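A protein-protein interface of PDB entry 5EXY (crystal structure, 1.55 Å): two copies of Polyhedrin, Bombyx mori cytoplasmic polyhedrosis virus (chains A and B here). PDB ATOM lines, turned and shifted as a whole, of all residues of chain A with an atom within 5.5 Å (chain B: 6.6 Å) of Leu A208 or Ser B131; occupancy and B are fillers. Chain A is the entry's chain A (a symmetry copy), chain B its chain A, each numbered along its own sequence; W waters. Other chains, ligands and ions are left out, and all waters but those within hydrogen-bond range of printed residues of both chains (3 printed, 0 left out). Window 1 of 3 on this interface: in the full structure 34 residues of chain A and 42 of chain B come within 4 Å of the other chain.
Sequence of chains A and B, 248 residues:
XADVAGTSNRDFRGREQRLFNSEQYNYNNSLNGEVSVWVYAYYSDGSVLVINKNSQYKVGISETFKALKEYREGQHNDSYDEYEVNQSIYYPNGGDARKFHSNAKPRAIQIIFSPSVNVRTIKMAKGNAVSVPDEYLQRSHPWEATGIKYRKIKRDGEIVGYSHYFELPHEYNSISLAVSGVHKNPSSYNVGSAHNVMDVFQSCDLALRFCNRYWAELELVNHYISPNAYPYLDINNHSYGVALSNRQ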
ATOM      1  N   ASN A  52     -15.603  -2.270  23.692  1.00  0.00           N
ATOM      2  CA  ASN A  52     -15.294  -1.071  22.943  1.00  0.00           C
ATOM      3  C   ASN A  52     -16.441  -0.121  23.066  1.00  0.00           C
ATOM      4  O   ASN A  52     -17.591  -0.551  22.975  1.00  0.00           O
ATOM      5  CB  ASN A  52     -15.083  -1.454  21.479  1.00  0.00           C
ATOM      6  CG  ASN A  52     -14.968  -0.354  20.452  1.00  0.00           C
ATOM      7  OD1 ASN A  52     -15.508  -0.480  19.349  1.00  0.00           O
ATOM      8  ND2 ASN A  52     -14.295   0.734  20.730  1.00  0.00           N
ATOM      9  N   LYS A  53     -16.138   1.169  23.155  1.00  0.00           N
ATOM     10  CA  LYS A  53     -17.170   2.203  23.075  1.00  0.00           C
ATOM     11  C   LYS A  53     -16.656   3.252  22.127  1.00  0.00           C
ATOM     12  O   LYS A  53     -15.481   3.630  22.186  1.00  0.00           O
ATOM     13  CB  LYS A  53     -17.531   2.799  24.439  1.00  0.00           C
ATOM     14  CG  LYS A  53     -18.881   3.544  24.295  1.00  0.00           C
ATOM     15  CD  LYS A  53     -19.503   3.947  25.547  1.00  0.00           C
ATOM     16  CE  LYS A  53     -20.044   2.831  26.388  1.00  0.00           C
ATOM     17  NZ  LYS A  53     -20.195   3.290  27.783  1.00  0.00           N
ATOM     18  N   ASN A  54     -17.530   3.646  21.184  1.00  0.00           N
ATOM     19  CA  ASN A  54     -17.250   4.639  20.158  1.00  0.00           C
ATOM     20  C   ASN A  54     -18.252   5.755  20.261  1.00  0.00           C
ATOM     21  O   ASN A  54     -19.456   5.496  20.143  1.00  0.00           O
ATOM     22  CB  ASN A  54     -17.387   3.983  18.787  1.00  0.00           C
ATOM     23  CG  ASN A  54     -16.475   2.799  18.636  1.00  0.00           C
ATOM     24  OD1 ASN A  54     -15.261   2.895  18.920  1.00  0.00           O
ATOM     25  ND2 ASN A  54     -17.011   1.650  18.241  1.00  0.00           N
ATOM     26  N   SER A  55     -17.784   7.018  20.424  1.00  0.00           N
ATOM     27  CA  SER A  55     -18.729   8.119  20.526  1.00  0.00           C
ATOM     28  C   SER A  55     -18.103   9.431  20.144  1.00  0.00           C
ATOM     29  O   SER A  55     -16.884   9.612  20.227  1.00  0.00           O
ATOM     30  CB  SER A  55     -19.241   8.216  21.954  1.00  0.00           C
ATOM     31  OG  SER A  55     -20.427   9.020  21.933  1.00  0.00           O
ATOM     32  N   LEU A 206     -26.043   8.096  21.857  1.00  0.00           N
ATOM     33  CA  LEU A 206     -25.693   7.563  20.548  1.00  0.00           C
ATOM     34  C   LEU A 206     -24.429   6.724  20.601  1.00  0.00           C
ATOM     35  O   LEU A 206     -24.104   6.090  19.603  1.00  0.00           O
ATOM     36  CB  LEU A 206     -25.533   8.727  19.557  1.00  0.00           C
ATOM     37  CG  LEU A 206     -26.812   9.480  19.258  1.00  0.00           C
ATOM     38  CD1 LEU A 206     -26.512  10.855  18.754  1.00  0.00           C
ATOM     39  CD2 LEU A 206     -27.695   8.702  18.306  1.00  0.00           C
ATOM     40  N   ALA A 207     -23.702   6.751  21.740  1.00  0.00           N
ATOM     41  CA  ALA A 207     -22.447   5.988  21.841  1.00  0.00           C
ATOM     42  C   ALA A 207     -22.752   4.554  21.531  1.00  0.00           C
ATOM     43  O   ALA A 207     -23.713   4.010  22.089  1.00  0.00           O
ATOM     44  CB  ALA A 207     -21.857   6.099  23.218  1.00  0.00           C
ATOM     45  N   LEU A 208     -21.927   3.916  20.696  1.00  0.00           N
ATOM     46  CA  LEU A 208     -22.128   2.502  20.372  1.00  0.00           C
ATOM     47  C   LEU A 208     -21.133   1.662  21.154  1.00  0.00           C
ATOM     48  O   LEU A 208     -19.962   2.023  21.252  1.00  0.00           O
ATOM     49  CB  LEU A 208     -21.993   2.174  18.883  1.00  0.00           C
ATOM     50  CG  LEU A 208     -22.994   2.839  17.945  1.00  0.00           C
ATOM     51  CD1 LEU A 208     -22.614   2.591  16.525  1.00  0.00           C
ATOM     52  CD2 LEU A 208     -24.400   2.357  18.176  1.00  0.00           C
ATOM     53  N   ARG A 209     -21.610   0.537  21.699  1.00  0.00           N
ATOM     54  CA  ARG A 209     -20.799  -0.376  22.514  1.00  0.00           C
ATOM     55  C   ARG A 209     -20.654  -1.690  21.769  1.00  0.00           C
ATOM     56  O   ARG A 209     -21.523  -2.079  21.002  1.00  0.00           O
ATOM     57  CB  ARG A 209     -21.488  -0.625  23.867  1.00  0.00           C
ATOM     58  CG  ARG A 209     -20.708  -1.517  24.847  1.00  0.00           C
ATOM     59  CD  ARG A 209     -21.393  -1.499  26.196  1.00  0.00           C
ATOM     60  NE  ARG A 209     -20.654  -2.242  27.232  1.00  0.00           N
ATOM     61  CZ  ARG A 209     -20.696  -3.561  27.388  1.00  0.00           C
ATOM     62  NH1 ARG A 209     -21.425  -4.314  26.570  1.00  0.00           N
ATOM     63  NH2 ARG A 209     -20.006  -4.140  28.356  1.00  0.00           N
ATOM     64  N   PHE A 210     -19.548  -2.368  21.989  1.00  0.00           N
ATOM     65  CA  PHE A 210     -19.314  -3.707  21.457  1.00  0.00           C
ATOM     66  C   PHE A 210     -18.617  -4.517  22.539  1.00  0.00           C
ATOM     67  O   PHE A 210     -17.734  -4.003  23.214  1.00  0.00           O
ATOM     68  CB  PHE A 210     -18.425  -3.680  20.235  1.00  0.00           C
ATOM     69  CG  PHE A 210     -18.009  -5.042  19.745  1.00  0.00           C
ATOM     70  CD1 PHE A 210     -18.876  -5.819  18.991  1.00  0.00           C
ATOM     71  CD2 PHE A 210     -16.773  -5.563  20.063  1.00  0.00           C
ATOM     72  CE1 PHE A 210     -18.476  -7.082  18.513  1.00  0.00           C
ATOM     73  CE2 PHE A 210     -16.387  -6.838  19.622  1.00  0.00           C
ATOM     74  CZ  PHE A 210     -17.230  -7.580  18.823  1.00  0.00           C
ATOM     75  N   SER B  62     -29.463   2.647  22.974  1.00  0.00           N
ATOM     76  CA  SER B  62     -28.276   2.171  22.254  1.00  0.00           C
ATOM     77  C   SER B  62     -28.139   0.708  22.531  1.00  0.00           C
ATOM     78  O   SER B  62     -28.120   0.315  23.698  1.00  0.00           O
ATOM     79  CB  SER B  62     -27.015   2.875  22.724  1.00  0.00           C
ATOM     80  OG  SER B  62     -25.915   2.391  21.962  1.00  0.00           O
ATOM     81  N   GLU B  63     -28.073  -0.107  21.481  1.00  0.00           N
ATOM     82  CA  GLU B  63     -27.973  -1.548  21.652  1.00  0.00           C
ATOM     83  C   GLU B  63     -26.917  -2.111  20.706  1.00  0.00           C
ATOM     84  O   GLU B  63     -26.729  -1.623  19.602  1.00  0.00           O
ATOM     85  CB  GLU B  63     -29.312  -2.183  21.341  1.00  0.00           C
ATOM     86  CG  GLU B  63     -30.465  -1.729  22.235  1.00  0.00           C
ATOM     87  CD  GLU B  63     -30.339  -2.054  23.718  1.00  0.00           C
ATOM     88  OE1 GLU B  63     -29.644  -3.038  24.064  1.00  0.00           O
ATOM     89  OE2 GLU B  63     -30.939  -1.322  24.540  1.00  0.00           O
ATOM     90  N   THR B  64     -26.278  -3.193  21.128  1.00  0.00           N
ATOM     91  CA  THR B  64     -25.322  -3.901  20.312  1.00  0.00           C
ATOM     92  C   THR B  64     -26.047  -4.812  19.333  1.00  0.00           C
ATOM     93  O   THR B  64     -27.254  -5.108  19.511  1.00  0.00           O
ATOM     94  CB  THR B  64     -24.462  -4.791  21.202  1.00  0.00           C
ATOM     95  OG1 THR B  64     -25.293  -5.768  21.813  1.00  0.00           O
ATOM     96  CG2 THR B  64     -23.796  -4.004  22.321  1.00  0.00           C
ATOM     97  N   PHE B  65     -25.293  -5.359  18.371  1.00  0.00           N
ATOM     98  CA  PHE B  65     -25.841  -6.360  17.447  1.00  0.00           C
ATOM     99  C   PHE B  65     -26.419  -7.495  18.278  1.00  0.00           C
ATOM    100  O   PHE B  65     -27.562  -7.936  18.034  1.00  0.00           O
ATOM    101  CB  PHE B  65     -24.755  -6.866  16.441  1.00  0.00           C
ATOM    102  CG  PHE B  65     -25.151  -8.108  15.695  1.00  0.00           C
ATOM    103  CD1 PHE B  65     -26.030  -8.042  14.607  1.00  0.00           C
ATOM    104  CD2 PHE B  65     -24.759  -9.355  16.148  1.00  0.00           C
ATOM    105  CE1 PHE B  65     -26.581  -9.201  14.072  1.00  0.00           C
ATOM    106  CE2 PHE B  65     -25.204 -10.517  15.509  1.00  0.00           C
ATOM    107  CZ  PHE B  65     -26.125 -10.435  14.490  1.00  0.00           C
ATOM    108  N   ALA B 125     -27.495   6.354  15.006  1.00  0.00           N
ATOM    109  CA  ALA B 125     -26.224   5.723  14.680  1.00  0.00           C
ATOM    110  C   ALA B 125     -26.579   4.256  14.358  1.00  0.00           C
ATOM    111  O   ALA B 125     -26.829   3.482  15.282  1.00  0.00           O
ATOM    112  CB  ALA B 125     -25.302   5.771  15.869  1.00  0.00           C
ATOM    113  N   LYS B 126     -26.639   3.889  13.062  1.00  0.00           N
ATOM    114  CA  LYS B 126     -26.933   2.537  12.610  1.00  0.00           C
ATOM    115  C   LYS B 126     -25.609   1.983  12.190  1.00  0.00           C
ATOM    116  O   LYS B 126     -25.134   2.279  11.095  1.00  0.00           O
ATOM    117  CB  LYS B 126     -27.949   2.543  11.455  1.00  0.00           C
ATOM    118  CG  LYS B 126     -28.281   1.144  10.977  1.00  0.00           C
ATOM    119  CD  LYS B 126     -29.477   1.099   9.987  1.00  0.00           C
ATOM    120  CE  LYS B 126     -29.104   1.468   8.570  1.00  0.00           C
ATOM    121  NZ  LYS B 126     -28.460   0.341   7.832  1.00  0.00           N
ATOM    122  N   GLY B 127     -24.977   1.267  13.090  1.00  0.00           N
ATOM    123  CA  GLY B 127     -23.647   0.742  12.848  1.00  0.00           C
ATOM    124  C   GLY B 127     -23.618  -0.650  12.263  1.00  0.00           C
ATOM    125  O   GLY B 127     -24.641  -1.304  12.076  1.00  0.00           O
ATOM    126  N   ASN B 128     -22.416  -1.097  11.971  1.00  0.00           N
ATOM    127  CA  ASN B 128     -22.237  -2.470  11.524  1.00  0.00           C
ATOM    128  C   ASN B 128     -22.245  -3.397  12.763  1.00  0.00           C
ATOM    129  O   ASN B 128     -22.455  -2.945  13.903  1.00  0.00           O
ATOM    130  CB  ASN B 128     -20.971  -2.625  10.688  1.00  0.00           C
ATOM    131  CG  ASN B 128     -19.702  -2.374  11.451  1.00  0.00           C
ATOM    132  OD1 ASN B 128     -19.698  -2.282  12.683  1.00  0.00           O
ATOM    133  ND2 ASN B 128     -18.601  -2.178  10.735  1.00  0.00           N
ATOM    134  N   ALA B 129     -22.010  -4.702  12.549  1.00  0.00           N
ATOM    135  CA  ALA B 129     -22.117  -5.649  13.665  1.00  0.00           C
ATOM    136  C   ALA B 129     -21.063  -5.472  14.761  1.00  0.00           C
ATOM    137  O   ALA B 129     -21.259  -6.011  15.856  1.00  0.00           O
ATOM    138  CB  ALA B 129     -22.113  -7.074  13.172  1.00  0.00           C
ATOM    139  N   VAL B 130     -19.942  -4.747  14.472  1.00  0.00           N
ATOM    140  CA  VAL B 130     -18.929  -4.462  15.485  1.00  0.00           C
ATOM    141  C   VAL B 130     -19.041  -3.028  16.029  1.00  0.00           C
ATOM    142  O   VAL B 130     -18.116  -2.544  16.680  1.00  0.00           O
ATOM    143  CB  VAL B 130     -17.501  -4.796  15.052  1.00  0.00           C
ATOM    144  CG1 VAL B 130     -17.334  -6.291  14.880  1.00  0.00           C
ATOM    145  CG2 VAL B 130     -17.106  -4.052  13.763  1.00  0.00           C
ATOM    146  N   SER B 131     -20.180  -2.375  15.809  1.00  0.00           N
ATOM    147  CA  SER B 131     -20.524  -1.128  16.456  1.00  0.00           C
ATOM    148  C   SER B 131     -19.746   0.043  15.946  1.00  0.00           C
ATOM    149  O   SER B 131     -19.422   0.957  16.703  1.00  0.00           O
ATOM    150  CB  SER B 131     -20.435  -1.264  17.967  1.00  0.00           C
ATOM    151  OG  SER B 131     -21.346  -2.256  18.418  1.00  0.00           O
ATOM    152  N   VAL B 132     -19.520   0.054  14.608  1.00  0.00           N
ATOM    153  CA  VAL B 132     -18.880   1.159  13.920  1.00  0.00           C
ATOM    154  C   VAL B 132     -19.945   1.805  13.012  1.00  0.00           C
ATOM    155  O   VAL B 132     -20.578   1.092  12.210  1.00  0.00           O
ATOM    156  CB  VAL B 132     -17.713   0.652  13.094  1.00  0.00           C
ATOM    157  CG1 VAL B 132     -17.167   1.749  12.198  1.00  0.00           C
ATOM    158  CG2 VAL B 132     -16.618   0.121  14.014  1.00  0.00           C
ATOM    159  N   PRO B 133     -20.166   3.140  13.109  1.00  0.00           N
ATOM    160  CA  PRO B 133     -21.272   3.741  12.346  1.00  0.00           C
ATOM    161  C   PRO B 133     -21.142   3.635  10.843  1.00  0.00           C
ATOM    162  O   PRO B 133     -22.159   3.454  10.177  1.00  0.00           O
ATOM    163  CB  PRO B 133     -21.242   5.205  12.776  1.00  0.00           C
ATOM    164  CG  PRO B 133     -20.690   5.203  14.090  1.00  0.00           C
ATOM    165  CD  PRO B 133     -19.634   4.103  14.089  1.00  0.00           C
ATOM    166  N   LEU B 137     -13.981   3.496  11.733  1.00  0.00           N
ATOM    167  CA  LEU B 137     -14.101   4.581  12.697  1.00  0.00           C
ATOM    168  C   LEU B 137     -13.574   5.896  12.176  1.00  0.00           C
ATOM    169  O   LEU B 137     -14.196   6.930  12.405  1.00  0.00           O
ATOM    170  CB  LEU B 137     -13.375   4.253  13.994  1.00  0.00           C
ATOM    171  CG  LEU B 137     -14.008   3.167  14.885  1.00  0.00           C
ATOM    172  CD1 LEU B 137     -13.085   2.826  16.008  1.00  0.00           C
ATOM    173  CD2 LEU B 137     -15.298   3.621  15.465  1.00  0.00           C
ATOM    174  N   PRO B 142     -20.535  10.151  13.770  1.00  0.00           N
ATOM    175  CA  PRO B 142     -21.187   9.266  14.758  1.00  0.00           C
ATOM    176  C   PRO B 142     -22.710   9.127  14.714  1.00  0.00           C
ATOM    177  O   PRO B 142     -23.295   8.402  15.553  1.00  0.00           O
ATOM    178  CB  PRO B 142     -20.740   9.853  16.091  1.00  0.00           C
ATOM    179  CG  PRO B 142     -19.471  10.543  15.769  1.00  0.00           C
ATOM    180  CD  PRO B 142     -19.753  11.196  14.464  1.00  0.00           C
ATOM    181  N   SER B 176     -25.851  -2.752  14.559  1.00  0.00           N
ATOM    182  CA  SER B 176     -25.894  -2.202  15.909  1.00  0.00           C
ATOM    183  C   SER B 176     -26.720  -0.926  15.762  1.00  0.00           C
ATOM    184  O   SER B 176     -26.870  -0.406  14.641  1.00  0.00           O
ATOM    185  CB  SER B 176     -24.501  -1.894  16.442  1.00  0.00           C
ATOM    186  OG  SER B 176     -23.779  -1.093  15.539  1.00  0.00           O
ATOM    187  N   LEU B 177     -27.308  -0.418  16.856  1.00  0.00           N
ATOM    188  CA  LEU B 177     -28.205   0.712  16.644  1.00  0.00           C
ATOM    189  C   LEU B 177     -28.317   1.573  17.848  1.00  0.00           C
ATOM    190  O   LEU B 177     -28.545   1.054  18.949  1.00  0.00           O
ATOM    191  CB  LEU B 177     -29.609   0.128  16.336  1.00  0.00           C
ATOM    192  CG  LEU B 177     -30.706   1.170  16.080  1.00  0.00           C
ATOM    193  CD1 LEU B 177     -30.466   1.942  14.829  1.00  0.00           C
ATOM    194  CD2 LEU B 177     -32.080   0.511  15.966  1.00  0.00           C
ATOM    195  N   ALA B 178     -28.242   2.901  17.650  1.00  0.00           N
ATOM    196  CA  ALA B 178     -28.566   3.824  18.716  1.00  0.00           C
ATOM    197  C   ALA B 178     -29.393   4.942  18.121  1.00  0.00           C
ATOM    198  O   ALA B 178     -29.230   5.289  16.957  1.00  0.00           O
ATOM    199  CB  ALA B 178     -27.325   4.385  19.398  1.00  0.00           C
HETATM  200  O   HOH W   1     -15.673  -2.522  17.773  1.00  0.00           O
HETATM  201  O   HOH W   2     -24.509   0.016  21.524  1.00  0.00           O
HETATM  202  O   HOH W   3     -22.458   7.487  17.932  1.00  0.00           O
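Water W1 lies within hydrogen-bond range of OD1 of Asn A52 (2.6 Å) and O of Val B130 (2.7 Å).
Water W3 bridges the backbone carbonyl oxygen (O) of Pro B142 (2.7 Å) and the backbone carbonyl oxygen (O) of Leu A206 (2.7 Å).
Water W2 lies within hydrogen-bond range of OG of Ser B62, N of Arg A209 and O of Glu B63.
Hydrophobic or aromatic side chains of chain B within 4 Å of the printed part of chain A: Ala B125, Val B130, Leu B137 and Ala B178.
Of the 9 printed residues of chain A, 6 touch a printed residue of chain B.
Printed residues of chain A that touch a printed residue of chain B: Asn A54, Leu A206, Ala A207, Leu A208, Arg A209 and Phe A210.
Hydrophobic or aromatic side chains of chain A within 4 Å of the printed part of chain B: Leu A206, Leu A208 and Phe A210.
Of the printed residues of chain B, Leu A206 touches Ala B125 and Ala B178.
Of the printed residues of chain B, Leu A208 touches Ala B125, Ser B131, Ser B176 and Ala B178.
Of the printed residues of chain B, Phe A210 touches Ala B129, Val B130 and Ser B131.
Printed residues of chain A within 4 Å of Ala B125: Leu A206 and Leu A208.
Gly B127 touches none of the printed residues of chain A.
Ser B131 touches just these residues of chain A: Asn A54, Leu A208, Arg A209 and Phe A210.
Of the printed residues of chain A, Ser B176 touches Leu A208 (3.99 Å).
Of the printed residues of chain A, Ala B178 touches Leu A206 (3.7 Å) and Leu A208 (3.8 Å).
The nearest printed residue of chain B that does not touch Leu A208 is Leu B177 (4.01 Å).
The nearest residue of chain A that does not touch Ser B131 is Asn A52 (4.9 Å).
The side-chain hydroxyl (OG) of Ser B62 is in hydrogen-bond range of the backbone carbonyl oxygen (O) of Ala A207, 2.7 Å away.
O of Ser B131 lies within hydrogen-bond range of ND2 of Asn A54, at 2.9 Å.
O of Arg A209 is in hydrogen-bond range of OG of Ser B131 (2.6 Å).
OD1 of Asn B128 sits at hydrogen-bond distance from N of Ser B131 (3.2 Å).
OG of Ser B176 sits at hydrogen-bond distance from O of Asn B128, at 2.8 Å.
The backbone carbonyl oxygen of Ser B176 is in hydrogen-bond range of the backbone NH of Gly B127 (3.0 Å).
The backbone NH of Asn A54 is in hydrogen-bond range of the backbone carbonyl oxygen of Leu A208, 2.9 Å away.
OD1 of Asn B128 is in hydrogen-bond range of N of Val B130.
The backbone carbonyl oxygen (O) of Ala B125 lies within hydrogen-bond range of the backbone NH (N) of Ala B178 (2.8 Å).
No position is printed for both chains.
Leu B137 touches Asn A54 (CD2 to CG, 3.5 Å).
Leu A206 touches Ala B125.
O of Leu A206 touches CB of Ala B178 (3.7 Å).
Leu A208 touches Ala B125 (CD2 to O, 3.9 Å).
Ser B131 touches Leu A208.
OG of Ser B176 touches CD1 of Leu A208, at 3.99 Å.
Arg A209 touches Thr B64 (O to CG2, 3.3 Å).
Phe A210 touches Ala B129 (CD1 to O, 3.9 Å).
CB of Phe A210 touches O of Val B130, at 3.7 Å.
Phe A210 touches Ser B131.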
